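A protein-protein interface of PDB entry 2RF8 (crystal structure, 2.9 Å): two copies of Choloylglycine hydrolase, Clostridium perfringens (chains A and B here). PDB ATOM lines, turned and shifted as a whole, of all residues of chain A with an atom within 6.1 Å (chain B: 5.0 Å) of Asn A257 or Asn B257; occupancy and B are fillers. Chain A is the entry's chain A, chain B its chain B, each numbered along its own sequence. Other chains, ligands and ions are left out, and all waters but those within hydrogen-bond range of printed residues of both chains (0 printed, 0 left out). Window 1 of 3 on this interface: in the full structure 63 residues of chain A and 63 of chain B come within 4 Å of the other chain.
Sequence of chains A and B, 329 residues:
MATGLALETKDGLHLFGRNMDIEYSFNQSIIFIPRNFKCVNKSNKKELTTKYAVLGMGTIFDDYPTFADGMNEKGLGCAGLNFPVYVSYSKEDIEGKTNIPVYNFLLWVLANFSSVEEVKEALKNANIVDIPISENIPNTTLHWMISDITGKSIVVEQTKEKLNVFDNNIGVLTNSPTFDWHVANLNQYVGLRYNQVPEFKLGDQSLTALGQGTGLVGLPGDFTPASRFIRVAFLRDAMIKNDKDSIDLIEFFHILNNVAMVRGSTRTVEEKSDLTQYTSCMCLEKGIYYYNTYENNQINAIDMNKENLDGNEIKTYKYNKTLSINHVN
O of Phe B253 lies within hydrogen-bond range of ND2 of Asn B257 (2.8 Å). OD1 of Asn A257 sits close to O of Phe A253, at 3.0 Å.
OD1 of Asn B257 touches OD1 of Asn A257, at 3.8 Å. Asn B258 touches Asn A258 (ND2 to O, 3.7 Å).
Asn A257 touches just one residue of chain B: Asn B257 (3.8 Å). Asn B257 touches just one residue of chain A: Asn A257 (3.8 Å). Of the printed residues of chain A, Asn B258 touches Asn A258. Of the printed residues of chain B, Asn A258 touches Asn B258 (3.7 Å). Ile A255 touches none of the printed residues of chain B. Val A259 touches none of the printed residues of chain B.
Printed residues of chain B that touch a printed residue of chain A: Asn B257 and Asn B258. Of the 13 printed residues of chain A, 2 touch a printed residue of chain B. Among the printed residues, 2 pairs touch across the chains.
Asn A257 touches its own counterpart, Asn B257. Asn B258 touches its own counterpart, Asn A258. Of the 2 pairs that touch across the chains among the printed residues, 2 have their exchanged pair printed and touching as well.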
ATOM      1  N   ASN A  19     -10.352   9.723  13.031  1.00  0.00           N
ATOM      2  CA  ASN A  19     -11.004  11.020  13.175  1.00  0.00           C
ATOM      3  C   ASN A  19     -12.475  10.798  13.482  1.00  0.00           C
ATOM      4  O   ASN A  19     -13.156  10.083  12.751  1.00  0.00           O
ATOM      5  CB  ASN A  19     -10.902  11.824  11.876  1.00  0.00           C
ATOM      6  CG  ASN A  19      -9.664  12.696  11.809  1.00  0.00           C
ATOM      7  OD1 ASN A  19      -8.787  12.633  12.670  1.00  0.00           O
ATOM      8  ND2 ASN A  19      -9.590  13.523  10.774  1.00  0.00           N
ATOM      9  N   PHE A 252       1.128  10.806  11.881  1.00  0.00           N
ATOM     10  CA  PHE A 252      -0.225  10.258  11.926  1.00  0.00           C
ATOM     11  C   PHE A 252      -1.264  11.378  11.934  1.00  0.00           C
ATOM     12  O   PHE A 252      -2.280  11.300  11.238  1.00  0.00           O
ATOM     13  CB  PHE A 252      -0.389   9.382  13.174  1.00  0.00           C
ATOM     14  CG  PHE A 252      -1.637   8.544  13.180  1.00  0.00           C
ATOM     15  CD1 PHE A 252      -2.843   9.066  13.637  1.00  0.00           C
ATOM     16  CD2 PHE A 252      -1.601   7.221  12.752  1.00  0.00           C
ATOM     17  CE1 PHE A 252      -3.994   8.289  13.650  1.00  0.00           C
ATOM     18  CE2 PHE A 252      -2.748   6.437  12.762  1.00  0.00           C
ATOM     19  CZ  PHE A 252      -3.946   6.974  13.207  1.00  0.00           C
ATOM     20  N   PHE A 253      -0.994  12.417  12.720  1.00  0.00           N
ATOM     21  CA  PHE A 253      -1.907  13.548  12.863  1.00  0.00           C
ATOM     22  C   PHE A 253      -1.902  14.477  11.648  1.00  0.00           C
ATOM     23  O   PHE A 253      -2.944  15.020  11.284  1.00  0.00           O
ATOM     24  CB  PHE A 253      -1.606  14.323  14.147  1.00  0.00           C
ATOM     25  CG  PHE A 253      -2.065  13.624  15.396  1.00  0.00           C
ATOM     26  CD1 PHE A 253      -1.277  12.641  15.993  1.00  0.00           C
ATOM     27  CD2 PHE A 253      -3.284  13.946  15.978  1.00  0.00           C
ATOM     28  CE1 PHE A 253      -1.702  11.989  17.150  1.00  0.00           C
ATOM     29  CE2 PHE A 253      -3.715  13.302  17.135  1.00  0.00           C
ATOM     30  CZ  PHE A 253      -2.925  12.321  17.721  1.00  0.00           C
ATOM     31  N   HIS A 254      -0.736  14.644  11.024  1.00  0.00           N
ATOM     32  CA  HIS A 254      -0.606  15.463   9.814  1.00  0.00           C
ATOM     33  C   HIS A 254      -1.484  14.960   8.672  1.00  0.00           C
ATOM     34  O   HIS A 254      -2.125  15.752   7.978  1.00  0.00           O
ATOM     35  CB  HIS A 254       0.852  15.537   9.356  1.00  0.00           C
ATOM     36  CG  HIS A 254       1.687  16.484  10.157  1.00  0.00           C
ATOM     37  ND1 HIS A 254       1.491  17.848  10.136  1.00  0.00           N
ATOM     38  CD2 HIS A 254       2.720  16.266  11.004  1.00  0.00           C
ATOM     39  CE1 HIS A 254       2.363  18.430  10.939  1.00  0.00           C
ATOM     40  NE2 HIS A 254       3.124  17.492  11.474  1.00  0.00           N
ATOM     41  N   ILE A 255      -1.508  13.641   8.494  1.00  0.00           N
ATOM     42  CA  ILE A 255      -2.315  13.001   7.458  1.00  0.00           C
ATOM     43  C   ILE A 255      -3.802  13.224   7.729  1.00  0.00           C
ATOM     44  O   ILE A 255      -4.536  13.669   6.846  1.00  0.00           O
ATOM     45  CB  ILE A 255      -2.006  11.482   7.350  1.00  0.00           C
ATOM     46  CG1 ILE A 255      -0.549  11.254   6.928  1.00  0.00           C
ATOM     47  CG2 ILE A 255      -2.952  10.803   6.368  1.00  0.00           C
ATOM     48  CD1 ILE A 255      -0.034   9.848   7.187  1.00  0.00           C
ATOM     49  N   LEU A 256      -4.229  12.938   8.957  1.00  0.00           N
ATOM     50  CA  LEU A 256      -5.637  13.056   9.336  1.00  0.00           C
ATOM     51  C   LEU A 256      -6.136  14.494   9.425  1.00  0.00           C
ATOM     52  O   LEU A 256      -7.316  14.751   9.182  1.00  0.00           O
ATOM     53  CB  LEU A 256      -5.926  12.307  10.642  1.00  0.00           C
ATOM     54  CG  LEU A 256      -5.949  10.774  10.603  1.00  0.00           C
ATOM     55  CD1 LEU A 256      -6.417  10.231  11.937  1.00  0.00           C
ATOM     56  CD2 LEU A 256      -6.835  10.240   9.482  1.00  0.00           C
ATOM     57  N   ASN A 257      -5.249  15.429   9.767  1.00  0.00           N
ATOM     58  CA  ASN A 257      -5.620  16.846   9.819  1.00  0.00           C
ATOM     59  C   ASN A 257      -6.118  17.357   8.472  1.00  0.00           C
ATOM     60  O   ASN A 257      -7.040  18.171   8.413  1.00  0.00           O
ATOM     61  CB  ASN A 257      -4.459  17.713  10.314  1.00  0.00           C
ATOM     62  CG  ASN A 257      -4.228  17.594  11.813  1.00  0.00           C
ATOM     63  OD1 ASN A 257      -3.119  17.816  12.293  1.00  0.00           O
ATOM     64  ND2 ASN A 257      -5.269  17.239  12.557  1.00  0.00           N
ATOM     65  N   ASN A 258      -5.510  16.856   7.398  1.00  0.00           N
ATOM     66  CA  ASN A 258      -5.894  17.205   6.033  1.00  0.00           C
ATOM     67  C   ASN A 258      -7.348  16.854   5.699  1.00  0.00           C
ATOM     68  O   ASN A 258      -7.991  17.538   4.902  1.00  0.00           O
ATOM     69  CB  ASN A 258      -4.934  16.555   5.034  1.00  0.00           C
ATOM     70  CG  ASN A 258      -5.272  16.886   3.595  1.00  0.00           C
ATOM     71  OD1 ASN A 258      -6.079  16.206   2.964  1.00  0.00           O
ATOM     72  ND2 ASN A 258      -4.646  17.929   3.065  1.00  0.00           N
ATOM     73  N   VAL A 259      -7.856  15.787   6.314  1.00  0.00           N
ATOM     74  CA  VAL A 259      -9.242  15.359   6.103  1.00  0.00           C
ATOM     75  C   VAL A 259     -10.159  15.728   7.275  1.00  0.00           C
ATOM     76  O   VAL A 259     -11.303  15.277   7.342  1.00  0.00           O
ATOM     77  CB  VAL A 259      -9.343  13.842   5.791  1.00  0.00           C
ATOM     78  CG1 VAL A 259      -8.798  13.543   4.401  1.00  0.00           C
ATOM     79  CG2 VAL A 259      -8.623  13.016   6.847  1.00  0.00           C
ATOM     80  N   ALA A 260      -9.655  16.556   8.186  1.00  0.00           N
ATOM     81  CA  ALA A 260     -10.432  16.988   9.346  1.00  0.00           C
ATOM     82  C   ALA A 260     -11.433  18.086   8.989  1.00  0.00           C
ATOM     83  O   ALA A 260     -11.115  19.009   8.233  1.00  0.00           O
ATOM     84  CB  ALA A 260      -9.514  17.445  10.466  1.00  0.00           C
ATOM     85  N   MET A 261     -12.640  17.970   9.539  1.00  0.00           N
ATOM     86  CA  MET A 261     -13.707  18.941   9.310  1.00  0.00           C
ATOM     87  C   MET A 261     -13.509  20.199  10.153  1.00  0.00           C
ATOM     88  O   MET A 261     -13.242  20.118  11.352  1.00  0.00           O
ATOM     89  CB  MET A 261     -15.071  18.318   9.615  1.00  0.00           C
ATOM     90  CG  MET A 261     -15.538  17.288   8.599  1.00  0.00           C
ATOM     91  SD  MET A 261     -17.176  16.649   8.997  1.00  0.00           S
ATOM     92  CE  MET A 261     -17.492  15.578   7.597  1.00  0.00           C
ATOM     93  N   THR A 279      -9.233  13.359  17.519  1.00  0.00           N
ATOM     94  CA  THR A 279      -8.388  12.477  16.726  1.00  0.00           C
ATOM     95  C   THR A 279      -7.579  11.586  17.660  1.00  0.00           C
ATOM     96  O   THR A 279      -6.750  12.071  18.432  1.00  0.00           O
ATOM     97  CB  THR A 279      -7.439  13.275  15.807  1.00  0.00           C
ATOM     98  OG1 THR A 279      -8.211  14.068  14.896  1.00  0.00           O
ATOM     99  CG2 THR A 279      -6.536  12.342  15.017  1.00  0.00           C
ATOM    100  N   ASN A 292      -6.137  13.885  20.699  1.00  0.00           N
ATOM    101  CA  ASN A 292      -6.379  15.310  20.890  1.00  0.00           C
ATOM    102  C   ASN A 292      -7.785  15.668  20.416  1.00  0.00           C
ATOM    103  O   ASN A 292      -8.392  14.914  19.657  1.00  0.00           O
ATOM    104  CB  ASN A 292      -5.307  16.160  20.193  1.00  0.00           C
ATOM    105  CG  ASN A 292      -5.420  16.147  18.673  1.00  0.00           C
ATOM    106  OD1 ASN A 292      -6.099  15.306  18.084  1.00  0.00           O
ATOM    107  ND2 ASN A 292      -4.738  17.089  18.031  1.00  0.00           N
ATOM    108  N   PHE B 253      -5.963  27.697  13.697  1.00  0.00           N
ATOM    109  CA  PHE B 253      -5.130  26.548  13.354  1.00  0.00           C
ATOM    110  C   PHE B 253      -5.869  25.497  12.530  1.00  0.00           C
ATOM    111  O   PHE B 253      -5.290  24.920  11.609  1.00  0.00           O
ATOM    112  CB  PHE B 253      -4.515  25.935  14.615  1.00  0.00           C
ATOM    113  CG  PHE B 253      -3.437  26.783  15.229  1.00  0.00           C
ATOM    114  CD1 PHE B 253      -3.759  27.820  16.103  1.00  0.00           C
ATOM    115  CD2 PHE B 253      -2.099  26.556  14.924  1.00  0.00           C
ATOM    116  CE1 PHE B 253      -2.764  28.613  16.666  1.00  0.00           C
ATOM    117  CE2 PHE B 253      -1.096  27.344  15.481  1.00  0.00           C
ATOM    118  CZ  PHE B 253      -1.430  28.375  16.355  1.00  0.00           C
ATOM    119  N   HIS B 254      -7.139  25.262  12.853  1.00  0.00           N
ATOM    120  CA  HIS B 254      -7.975  24.318  12.105  1.00  0.00           C
ATOM    121  C   HIS B 254      -8.087  24.684  10.624  1.00  0.00           C
ATOM    122  O   HIS B 254      -8.048  23.807   9.757  1.00  0.00           O
ATOM    123  CB  HIS B 254      -9.373  24.219  12.720  1.00  0.00           C
ATOM    124  CG  HIS B 254      -9.416  23.451  14.004  1.00  0.00           C
ATOM    125  ND1 HIS B 254      -9.221  22.088  14.061  1.00  0.00           N
ATOM    126  CD2 HIS B 254      -9.642  23.853  15.277  1.00  0.00           C
ATOM    127  CE1 HIS B 254      -9.317  21.685  15.316  1.00  0.00           C
ATOM    128  NE2 HIS B 254      -9.573  22.736  16.073  1.00  0.00           N
ATOM    129  N   ILE B 255      -8.226  25.982  10.350  1.00  0.00           N
ATOM    130  CA  ILE B 255      -8.342  26.498   8.985  1.00  0.00           C
ATOM    131  C   ILE B 255      -7.053  26.256   8.205  1.00  0.00           C
ATOM    132  O   ILE B 255      -7.090  25.764   7.075  1.00  0.00           O
ATOM    133  CB  ILE B 255      -8.701  28.011   8.967  1.00  0.00           C
ATOM    134  CG1 ILE B 255     -10.028  28.260   9.690  1.00  0.00           C
ATOM    135  CG2 ILE B 255      -8.783  28.536   7.539  1.00  0.00           C
ATOM    136  CD1 ILE B 255     -10.236  29.699  10.134  1.00  0.00           C
ATOM    137  N   LEU B 256      -5.918  26.589   8.819  1.00  0.00           N
ATOM    138  CA  LEU B 256      -4.618  26.439   8.168  1.00  0.00           C
ATOM    139  C   LEU B 256      -4.141  24.988   8.087  1.00  0.00           C
ATOM    140  O   LEU B 256      -3.326  24.653   7.225  1.00  0.00           O
ATOM    141  CB  LEU B 256      -3.559  27.324   8.837  1.00  0.00           C
ATOM    142  CG  LEU B 256      -3.646  28.840   8.605  1.00  0.00           C
ATOM    143  CD1 LEU B 256      -2.486  29.537   9.277  1.00  0.00           C
ATOM    144  CD2 LEU B 256      -3.682  29.197   7.119  1.00  0.00           C
ATOM    145  N   ASN B 257      -4.653  24.137   8.977  1.00  0.00           N
ATOM    146  CA  ASN B 257      -4.334  22.706   8.959  1.00  0.00           C
ATOM    147  C   ASN B 257      -4.791  22.024   7.672  1.00  0.00           C
ATOM    148  O   ASN B 257      -4.155  21.078   7.194  1.00  0.00           O
ATOM    149  CB  ASN B 257      -4.949  21.992  10.167  1.00  0.00           C
ATOM    150  CG  ASN B 257      -4.113  22.135  11.431  1.00  0.00           C
ATOM    151  OD1 ASN B 257      -4.304  21.391  12.393  1.00  0.00           O
ATOM    152  ND2 ASN B 257      -3.186  23.092  11.437  1.00  0.00           N
ATOM    153  N   ASN B 258      -5.898  22.520   7.121  1.00  0.00           N
ATOM    154  CA  ASN B 258      -6.467  21.996   5.885  1.00  0.00           C
ATOM    155  C   ASN B 258      -5.588  22.272   4.665  1.00  0.00           C
ATOM    156  O   ASN B 258      -5.521  21.453   3.747  1.00  0.00           O
ATOM    157  CB  ASN B 258      -7.879  22.552   5.679  1.00  0.00           C
ATOM    158  CG  ASN B 258      -8.525  22.041   4.411  1.00  0.00           C
ATOM    159  OD1 ASN B 258      -8.358  22.621   3.342  1.00  0.00           O
ATOM    160  ND2 ASN B 258      -9.272  20.950   4.524  1.00  0.00           N
ATOM    161  N   VAL B 259      -4.921  23.425   4.664  1.00  0.00           N
ATOM    162  CA  VAL B 259      -4.017  23.800   3.574  1.00  0.00           C
ATOM    163  C   VAL B 259      -2.549  23.536   3.926  1.00  0.00           C
ATOM    164  O   VAL B 259      -1.641  23.999   3.233  1.00  0.00           O
ATOM    165  CB  VAL B 259      -4.208  25.278   3.131  1.00  0.00           C
ATOM    166  CG1 VAL B 259      -5.570  25.472   2.470  1.00  0.00           C
ATOM    167  CG2 VAL B 259      -4.022  26.239   4.309  1.00  0.00           C
ATOM    168  N   ALA B 260      -2.329  22.787   5.005  1.00  0.00           N
ATOM    169  CA  ALA B 260      -0.983  22.418   5.433  1.00  0.00           C
ATOM    170  C   ALA B 260      -0.447  21.239   4.626  1.00  0.00           C
ATOM    171  O   ALA B 260      -1.155  20.254   4.400  1.00  0.00           O
ATOM    172  CB  ALA B 260      -0.961  22.104   6.920  1.00  0.00           C
